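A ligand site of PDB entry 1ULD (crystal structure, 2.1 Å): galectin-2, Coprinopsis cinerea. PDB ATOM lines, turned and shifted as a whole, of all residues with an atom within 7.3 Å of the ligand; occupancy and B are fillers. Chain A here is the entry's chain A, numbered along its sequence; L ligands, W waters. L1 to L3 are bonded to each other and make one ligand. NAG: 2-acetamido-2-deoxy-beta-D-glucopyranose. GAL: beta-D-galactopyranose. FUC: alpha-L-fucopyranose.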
ATOM      1  N   THR A  36     -28.849 -11.692  24.341  1.00  0.00           N
ATOM      2  CA  THR A  36     -27.411 -11.640  24.107  1.00  0.00           C
ATOM      3  C   THR A  36     -27.089 -12.140  22.694  1.00  0.00           C
ATOM      4  O   THR A  36     -27.523 -13.222  22.287  1.00  0.00           O
ATOM      5  CB  THR A  36     -26.681 -12.478  25.177  1.00  0.00           C
ATOM      6  OG1 THR A  36     -26.720 -11.771  26.430  1.00  0.00           O
ATOM      7  CG2 THR A  36     -25.233 -12.738  24.783  1.00  0.00           C
ATOM      8  N   VAL A  38     -23.951 -12.710  19.760  1.00  0.00           N
ATOM      9  CA  VAL A  38     -22.505 -12.823  19.598  1.00  0.00           C
ATOM     10  C   VAL A  38     -21.990 -12.952  18.176  1.00  0.00           C
ATOM     11  O   VAL A  38     -22.615 -13.579  17.328  1.00  0.00           O
ATOM     12  CB  VAL A  38     -21.981 -14.052  20.405  1.00  0.00           C
ATOM     13  CG1 VAL A  38     -20.489 -14.267  20.122  1.00  0.00           C
ATOM     14  CG2 VAL A  38     -22.217 -13.856  21.895  1.00  0.00           C
ATOM     15  N   HIS A  51     -14.071 -12.038  20.113  1.00  0.00           N
ATOM     16  CA  HIS A  51     -15.392 -12.397  20.591  1.00  0.00           C
ATOM     17  C   HIS A  51     -16.097 -11.098  20.958  1.00  0.00           C
ATOM     18  O   HIS A  51     -15.543 -10.272  21.683  1.00  0.00           O
ATOM     19  CB  HIS A  51     -15.238 -13.265  21.848  1.00  0.00           C
ATOM     20  CG  HIS A  51     -16.522 -13.591  22.541  1.00  0.00           C
ATOM     21  ND1 HIS A  51     -17.440 -14.495  22.038  1.00  0.00           N
ATOM     22  CD2 HIS A  51     -17.032 -13.160  23.721  1.00  0.00           C
ATOM     23  CE1 HIS A  51     -18.441 -14.615  22.886  1.00  0.00           C
ATOM     24  NE2 HIS A  51     -18.228 -13.814  23.915  1.00  0.00           N
ATOM     25  N   ILE A  52     -17.295 -10.899  20.434  1.00  0.00           N
ATOM     26  CA  ILE A  52     -18.071  -9.697  20.719  1.00  0.00           C
ATOM     27  C   ILE A  52     -19.424 -10.156  21.262  1.00  0.00           C
ATOM     28  O   ILE A  52     -20.273 -10.655  20.505  1.00  0.00           O
ATOM     29  CB  ILE A  52     -18.288  -8.839  19.460  1.00  0.00           C
ATOM     30  CG1 ILE A  52     -16.938  -8.490  18.838  1.00  0.00           C
ATOM     31  CG2 ILE A  52     -19.034  -7.550  19.824  1.00  0.00           C
ATOM     32  CD1 ILE A  52     -17.036  -7.777  17.509  1.00  0.00           C
ATOM     33  N   SER A  53     -19.620  -9.994  22.565  1.00  0.00           N
ATOM     34  CA  SER A  53     -20.843 -10.408  23.226  1.00  0.00           C
ATOM     35  C   SER A  53     -21.683  -9.181  23.551  1.00  0.00           C
ATOM     36  O   SER A  53     -21.367  -8.410  24.449  1.00  0.00           O
ATOM     37  CB  SER A  53     -20.512 -11.175  24.517  1.00  0.00           C
ATOM     38  OG  SER A  53     -21.684 -11.698  25.126  1.00  0.00           O
ATOM     39  N   ILE A  54     -22.761  -8.998  22.796  1.00  0.00           N
ATOM     40  CA  ILE A  54     -23.658  -7.857  22.977  1.00  0.00           C
ATOM     41  C   ILE A  54     -24.729  -8.295  23.968  1.00  0.00           C
ATOM     42  O   ILE A  54     -25.560  -9.156  23.661  1.00  0.00           O
ATOM     43  CB  ILE A  54     -24.258  -7.454  21.616  1.00  0.00           C
ATOM     44  CG1 ILE A  54     -23.115  -7.228  20.618  1.00  0.00           C
ATOM     45  CG2 ILE A  54     -25.104  -6.200  21.759  1.00  0.00           C
ATOM     46  CD1 ILE A  54     -23.540  -7.169  19.161  1.00  0.00           C
ATOM     47  N   ARG A  55     -24.713  -7.693  25.158  1.00  0.00           N
ATOM     48  CA  ARG A  55     -25.648  -8.057  26.214  1.00  0.00           C
ATOM     49  C   ARG A  55     -26.568  -6.912  26.633  1.00  0.00           C
ATOM     50  O   ARG A  55     -26.233  -6.120  27.529  1.00  0.00           O
ATOM     51  CB  ARG A  55     -24.864  -8.555  27.436  1.00  0.00           C
ATOM     52  CG  ARG A  55     -23.779  -9.575  27.095  1.00  0.00           C
ATOM     53  CD  ARG A  55     -22.970  -9.978  28.325  1.00  0.00           C
ATOM     54  NE  ARG A  55     -21.913 -10.943  28.001  1.00  0.00           N
ATOM     55  CZ  ARG A  55     -21.042 -11.405  28.895  1.00  0.00           C
ATOM     56  NH1 ARG A  55     -21.109 -11.009  30.158  1.00  0.00           N
ATOM     57  NH2 ARG A  55     -20.101 -12.276  28.522  1.00  0.00           N
ATOM     58  N   GLU A  58     -27.673  -6.817  30.334  1.00  0.00           N
ATOM     59  CA  GLU A  58     -26.605  -6.447  31.252  1.00  0.00           C
ATOM     60  C   GLU A  58     -26.107  -5.049  30.898  1.00  0.00           C
ATOM     61  O   GLU A  58     -25.276  -4.469  31.614  1.00  0.00           O
ATOM     62  CB  GLU A  58     -25.467  -7.461  31.097  1.00  0.00           C
ATOM     63  CG  GLU A  58     -24.549  -7.602  32.299  1.00  0.00           C
ATOM     64  CD  GLU A  58     -23.395  -8.544  32.025  1.00  0.00           C
ATOM     65  OE1 GLU A  58     -23.621  -9.599  31.370  1.00  0.00           O
ATOM     66  OE2 GLU A  58     -22.259  -8.242  32.463  1.00  0.00           O
ATOM     67  N   VAL A  60     -24.193  -4.178  28.463  1.00  0.00           N
ATOM     68  CA  VAL A  60     -22.765  -4.196  28.201  1.00  0.00           C
ATOM     69  C   VAL A  60     -22.443  -4.981  26.935  1.00  0.00           C
ATOM     70  O   VAL A  60     -23.238  -5.793  26.468  1.00  0.00           O
ATOM     71  CB  VAL A  60     -21.984  -4.829  29.383  1.00  0.00           C
ATOM     72  CG1 VAL A  60     -22.225  -6.337  29.427  1.00  0.00           C
ATOM     73  CG2 VAL A  60     -20.512  -4.519  29.272  1.00  0.00           C
ATOM     74  N   VAL A  62     -19.219  -7.209  25.642  1.00  0.00           N
ATOM     75  CA  VAL A  62     -17.960  -7.799  26.077  1.00  0.00           C
ATOM     76  C   VAL A  62     -17.088  -8.319  24.933  1.00  0.00           C
ATOM     77  O   VAL A  62     -17.570  -9.006  24.029  1.00  0.00           O
ATOM     78  CB  VAL A  62     -18.210  -8.966  27.056  1.00  0.00           C
ATOM     79  CG1 VAL A  62     -16.873  -9.482  27.616  1.00  0.00           C
ATOM     80  CG2 VAL A  62     -19.131  -8.516  28.191  1.00  0.00           C
ATOM     81  N   PHE A  63     -15.802  -7.966  24.991  1.00  0.00           N
ATOM     82  CA  PHE A  63     -14.832  -8.399  23.998  1.00  0.00           C
ATOM     83  C   PHE A  63     -13.837  -9.350  24.689  1.00  0.00           C
ATOM     84  O   PHE A  63     -13.464  -9.138  25.841  1.00  0.00           O
ATOM     85  CB  PHE A  63     -14.090  -7.197  23.427  1.00  0.00           C
ATOM     86  CG  PHE A  63     -14.981  -6.165  22.769  1.00  0.00           C
ATOM     87  CD1 PHE A  63     -15.623  -5.188  23.537  1.00  0.00           C
ATOM     88  CD2 PHE A  63     -15.204  -6.199  21.392  1.00  0.00           C
ATOM     89  CE1 PHE A  63     -16.455  -4.244  22.933  1.00  0.00           C
ATOM     90  CE2 PHE A  63     -16.037  -5.254  20.788  1.00  0.00           C
ATOM     91  CZ  PHE A  63     -16.665  -4.280  21.552  1.00  0.00           C
ATOM     92  N   ASN A  64     -13.441 -10.403  23.989  1.00  0.00           N
ATOM     93  CA  ASN A  64     -12.493 -11.360  24.559  1.00  0.00           C
ATOM     94  C   ASN A  64     -11.924 -12.235  23.445  1.00  0.00           C
ATOM     95  O   ASN A  64     -12.185 -11.994  22.259  1.00  0.00           O
ATOM     96  CB  ASN A  64     -13.195 -12.230  25.605  1.00  0.00           C
ATOM     97  CG  ASN A  64     -12.274 -12.617  26.770  1.00  0.00           C
ATOM     98  OD1 ASN A  64     -11.058 -12.761  26.595  1.00  0.00           O
ATOM     99  ND2 ASN A  64     -12.852 -12.808  27.950  1.00  0.00           N
ATOM    100  N   SER A  65     -11.138 -13.231  23.842  1.00  0.00           N
ATOM    101  CA  SER A  65     -10.520 -14.173  22.903  1.00  0.00           C
ATOM    102  C   SER A  65     -10.225 -15.466  23.654  1.00  0.00           C
ATOM    103  O   SER A  65     -10.323 -15.516  24.888  1.00  0.00           O
ATOM    104  CB  SER A  65      -9.206 -13.620  22.362  1.00  0.00           C
ATOM    105  OG  SER A  65      -9.338 -12.261  21.984  1.00  0.00           O
ATOM    106  N   ARG A  66      -9.860 -16.513  22.921  1.00  0.00           N
ATOM    107  CA  ARG A  66      -9.523 -17.801  23.515  1.00  0.00           C
ATOM    108  C   ARG A  66      -9.267 -18.828  22.427  1.00  0.00           C
ATOM    109  O   ARG A  66      -9.869 -18.783  21.352  1.00  0.00           O
ATOM    110  CB  ARG A  66     -10.657 -18.295  24.417  1.00  0.00           C
ATOM    111  CG  ARG A  66     -11.848 -18.901  23.682  1.00  0.00           C
ATOM    112  CD  ARG A  66     -12.924 -19.267  24.680  1.00  0.00           C
ATOM    113  NE  ARG A  66     -14.019 -20.044  24.103  1.00  0.00           N
ATOM    114  CZ  ARG A  66     -13.903 -21.273  23.621  1.00  0.00           C
ATOM    115  NH1 ARG A  66     -12.725 -21.894  23.631  1.00  0.00           N
ATOM    116  NH2 ARG A  66     -14.965 -21.891  23.109  1.00  0.00           N
ATOM    117  N   TRP A  72     -11.065 -18.135  28.262  1.00  0.00           N
ATOM    118  CA  TRP A  72     -11.206 -16.713  27.957  1.00  0.00           C
ATOM    119  C   TRP A  72     -10.124 -16.001  28.753  1.00  0.00           C
ATOM    120  O   TRP A  72      -9.670 -16.501  29.768  1.00  0.00           O
ATOM    121  CB  TRP A  72     -12.568 -16.168  28.423  1.00  0.00           C
ATOM    122  CG  TRP A  72     -13.761 -16.733  27.702  1.00  0.00           C
ATOM    123  CD1 TRP A  72     -14.731 -17.536  28.233  1.00  0.00           C
ATOM    124  CD2 TRP A  72     -14.121 -16.513  26.340  1.00  0.00           C
ATOM    125  NE1 TRP A  72     -15.666 -17.838  27.283  1.00  0.00           N
ATOM    126  CE2 TRP A  72     -15.328 -17.224  26.108  1.00  0.00           C
ATOM    127  CE3 TRP A  72     -13.545 -15.789  25.286  1.00  0.00           C
ATOM    128  CZ2 TRP A  72     -15.959 -17.227  24.857  1.00  0.00           C
ATOM    129  CZ3 TRP A  72     -14.181 -15.796  24.048  1.00  0.00           C
ATOM    130  CH2 TRP A  72     -15.378 -16.512  23.849  1.00  0.00           C
ATOM    131  N   GLY A  73      -9.709 -14.836  28.274  1.00  0.00           N
ATOM    132  CA  GLY A  73      -8.711 -14.073  28.985  1.00  0.00           C
ATOM    133  C   GLY A  73      -9.482 -13.016  29.743  1.00  0.00           C
ATOM    134  O   GLY A  73     -10.658 -13.216  30.044  1.00  0.00           O
ATOM    135  N   PRO A  74      -8.849 -11.891  30.101  1.00  0.00           N
ATOM    136  CA  PRO A  74      -9.628 -10.878  30.817  1.00  0.00           C
ATOM    137  C   PRO A  74     -10.616 -10.248  29.845  1.00  0.00           C
ATOM    138  O   PRO A  74     -10.371 -10.216  28.634  1.00  0.00           O
ATOM    139  CB  PRO A  74      -8.563  -9.890  31.299  1.00  0.00           C
ATOM    140  CG  PRO A  74      -7.490 -10.017  30.249  1.00  0.00           C
ATOM    141  CD  PRO A  74      -7.425 -11.504  30.024  1.00  0.00           C
ATOM    142  N   GLU A  75     -11.744  -9.771  30.355  1.00  0.00           N
ATOM    143  CA  GLU A  75     -12.744  -9.157  29.499  1.00  0.00           C
ATOM    144  C   GLU A  75     -12.507  -7.677  29.317  1.00  0.00           C
ATOM    145  O   GLU A  75     -11.924  -7.010  30.171  1.00  0.00           O
ATOM    146  CB  GLU A  75     -14.151  -9.331  30.081  1.00  0.00           C
ATOM    147  CG  GLU A  75     -14.566 -10.746  30.348  1.00  0.00           C
ATOM    148  CD  GLU A  75     -16.001 -10.818  30.822  1.00  0.00           C
ATOM    149  OE1 GLU A  75     -16.439  -9.862  31.506  1.00  0.00           O
ATOM    150  OE2 GLU A  75     -16.683 -11.815  30.529  1.00  0.00           O
ATOM    151  N   GLU A  76     -12.971  -7.167  28.191  1.00  0.00           N
ATOM    152  CA  GLU A  76     -12.879  -5.746  27.906  1.00  0.00           C
ATOM    153  C   GLU A  76     -14.332  -5.378  27.608  1.00  0.00           C
ATOM    154  O   GLU A  76     -14.978  -5.977  26.747  1.00  0.00           O
ATOM    155  CB  GLU A  76     -11.934  -5.496  26.742  1.00  0.00           C
ATOM    156  CG  GLU A  76     -10.493  -5.795  27.146  1.00  0.00           C
ATOM    157  CD  GLU A  76      -9.471  -5.403  26.106  1.00  0.00           C
ATOM    158  OE1 GLU A  76      -9.489  -4.231  25.665  1.00  0.00           O
ATOM    159  OE2 GLU A  76      -8.650  -6.270  25.732  1.00  0.00           O
ATOM    160  N   ARG A  77     -14.834  -4.396  28.357  1.00  0.00           N
ATOM    161  CA  ARG A  77     -16.228  -3.989  28.244  1.00  0.00           C
ATOM    162  C   ARG A  77     -16.481  -2.511  27.950  1.00  0.00           C
ATOM    163  O   ARG A  77     -15.617  -1.661  28.155  1.00  0.00           O
ATOM    164  CB  ARG A  77     -16.943  -4.332  29.552  1.00  0.00           C
ATOM    165  CG  ARG A  77     -16.787  -5.782  30.018  1.00  0.00           C
ATOM    166  CD  ARG A  77     -17.416  -5.976  31.399  1.00  0.00           C
ATOM    167  NE  ARG A  77     -17.795  -7.370  31.623  1.00  0.00           N
ATOM    168  CZ  ARG A  77     -18.965  -7.751  32.117  1.00  0.00           C
ATOM    169  NH1 ARG A  77     -19.892  -6.850  32.442  1.00  0.00           N
ATOM    170  NH2 ARG A  77     -19.223  -9.044  32.245  1.00  0.00           N
HETATM  171  C1  NAG L   1     -18.601 -13.904  34.825  1.00  0.00           C
HETATM  172  C2  NAG L   1     -18.314 -12.774  33.823  1.00  0.00           C
HETATM  173  C3  NAG L   1     -19.140 -13.032  32.566  1.00  0.00           C
HETATM  174  C4  NAG L   1     -18.791 -14.404  32.007  1.00  0.00           C
HETATM  175  C5  NAG L   1     -19.007 -15.487  33.081  1.00  0.00           C
HETATM  176  C6  NAG L   1     -18.591 -16.883  32.633  1.00  0.00           C
HETATM  177  C7  NAG L   1     -17.649 -10.664  34.751  1.00  0.00           C
HETATM  178  C8  NAG L   1     -18.033  -9.245  35.140  1.00  0.00           C
HETATM  179  N2  NAG L   1     -18.631 -11.487  34.396  1.00  0.00           N
HETATM  180  O1  NAG L   1     -17.839 -13.704  35.970  1.00  0.00           O
HETATM  181  O3  NAG L   1     -18.864 -12.033  31.594  1.00  0.00           O
HETATM  182  O4  NAG L   1     -19.604 -14.702  30.866  1.00  0.00           O
HETATM  183  O5  NAG L   1     -18.238 -15.166  34.262  1.00  0.00           O
HETATM  184  O6  NAG L   1     -17.251 -16.895  32.184  1.00  0.00           O
HETATM  185  O7  NAG L   1     -16.473 -11.013  34.783  1.00  0.00           O
HETATM  186  C1  GAL L   2     -18.948 -15.267  29.786  1.00  0.00           C
HETATM  187  C2  GAL L   2     -19.977 -15.778  28.779  1.00  0.00           C
HETATM  188  C3  GAL L   2     -19.296 -16.240  27.491  1.00  0.00           C
HETATM  189  C4  GAL L   2     -18.384 -15.134  26.949  1.00  0.00           C
HETATM  190  C5  GAL L   2     -17.392 -14.746  28.043  1.00  0.00           C
HETATM  191  C6  GAL L   2     -16.435 -13.653  27.606  1.00  0.00           C
HETATM  192  O2  GAL L   2     -20.713 -16.879  29.346  1.00  0.00           O
HETATM  193  O3  GAL L   2     -20.282 -16.574  26.520  1.00  0.00           O
HETATM  194  O4  GAL L   2     -19.175 -14.005  26.588  1.00  0.00           O
HETATM  195  O5  GAL L   2     -18.101 -14.268  29.207  1.00  0.00           O
HETATM  196  O6  GAL L   2     -15.515 -13.338  28.641  1.00  0.00           O
HETATM  197  C1  FUC L   3     -22.089 -16.887  29.098  1.00  0.00           C
HETATM  198  C2  FUC L   3     -22.704 -18.191  29.615  1.00  0.00           C
HETATM  199  C3  FUC L   3     -22.599 -18.219  31.142  1.00  0.00           C
HETATM  200  C4  FUC L   3     -23.281 -16.979  31.741  1.00  0.00           C
HETATM  201  C5  FUC L   3     -22.706 -15.705  31.121  1.00  0.00           C
HETATM  202  C6  FUC L   3     -23.486 -14.468  31.534  1.00  0.00           C
HETATM  203  O2  FUC L   3     -22.021 -19.293  29.063  1.00  0.00           O
HETATM  204  O3  FUC L   3     -23.233 -19.393  31.626  1.00  0.00           O
HETATM  205  O4  FUC L   3     -24.682 -17.039  31.497  1.00  0.00           O
HETATM  206  O5  FUC L   3     -22.766 -15.768  29.681  1.00  0.00           O
HETATM  207  O   HOH W   1     -23.325 -13.702  27.847  1.00  0.00           O
HETATM  208  O   HOH W   2     -21.423 -10.921  33.728  1.00  0.00           O
HETATM  209  O   HOH W   3     -14.734 -12.714  33.125  1.00  0.00           O
HETATM  210  O   HOH W   4     -22.016 -14.306  25.528  1.00  0.00           O
HETATM  211  O   HOH W   5     -17.462 -13.305  38.828  1.00  0.00           O
HETATM  212  O   HOH W   6     -19.752 -18.225  24.716  1.00  0.00           O
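The side-chain carboxylate (OE2) of Glu 75 is in hydrogen-bond range of an oxygen (O3) of NAG L1 (2.4 Å). The guanidinium group (NH2) of Arg 77 is in hydrogen-bond range of an oxygen (O3) of NAG L1 (3.1 Å). The side-chain amide nitrogen of Asn 64 lies within hydrogen-bond range of an oxygen (O6) of GAL L2, at 2.8 Å. An oxygen (O4) of GAL L2 sits at hydrogen-bond distance from a ring nitrogen (NE2) of His 51. An oxygen (O4) of GAL L2 lies within hydrogen-bond range of the guanidinium group (NH2) of Arg 55 (2.8 Å).
The backbone NH (N) of His 51 sits at hydrogen-bond distance from the backbone carbonyl oxygen (O) of Asn 64 (2.9 Å). NH1 of Arg 77 is in salt-bridge range of OE2 of Glu 58 (2.7 Å). OE1 of Glu 58 is in salt-bridge range of NH1 of Arg 55 (3.1 Å). The backbone NH (N) of Arg 55 is in hydrogen-bond range of the backbone carbonyl oxygen (O) of Val 60, 2.7 Å away. OG of Ser 53 sits at hydrogen-bond distance from NE of Arg 55 (3.0 Å). The side-chain amide oxygen (OD1) of Asn 64 sits at hydrogen-bond distance from the backbone NH (N) of Gly 73 (3.0 Å). NE of Arg 77 lies within salt-bridge range of OE1 of Glu 75 (2.8 Å). The backbone carbonyl oxygen (O) of Val 62 is in hydrogen-bond range of the backbone NH (N) of Ser 53 (2.7 Å).
Residues that only touch the ligand: Trp 72 and Ser 53. Hydrophobic or aromatic side chains within 4 Å of the ligand: His 51 and Trp 72. Of the 20 residues printed, 7 come within 4 Å of the ligand.
Water W1 lies within hydrogen-bond range of O5 of FUC L3 (2.8 Å) and NE of Arg 55 (3.1 Å). Water W2 lies within hydrogen-bond range of N2 of NAG L1, OE2 of Glu 58 and NH2 of Arg 77. Water W3 bridges an oxygen (O7) of NAG L1 (2.9 Å) and the side-chain carboxylate (OE2) of Glu 75 (3.4 Å). Water W4 lies within hydrogen-bond range of OG of Ser 53 (2.7 Å) and O3 of GAL L2 (3.0 Å).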
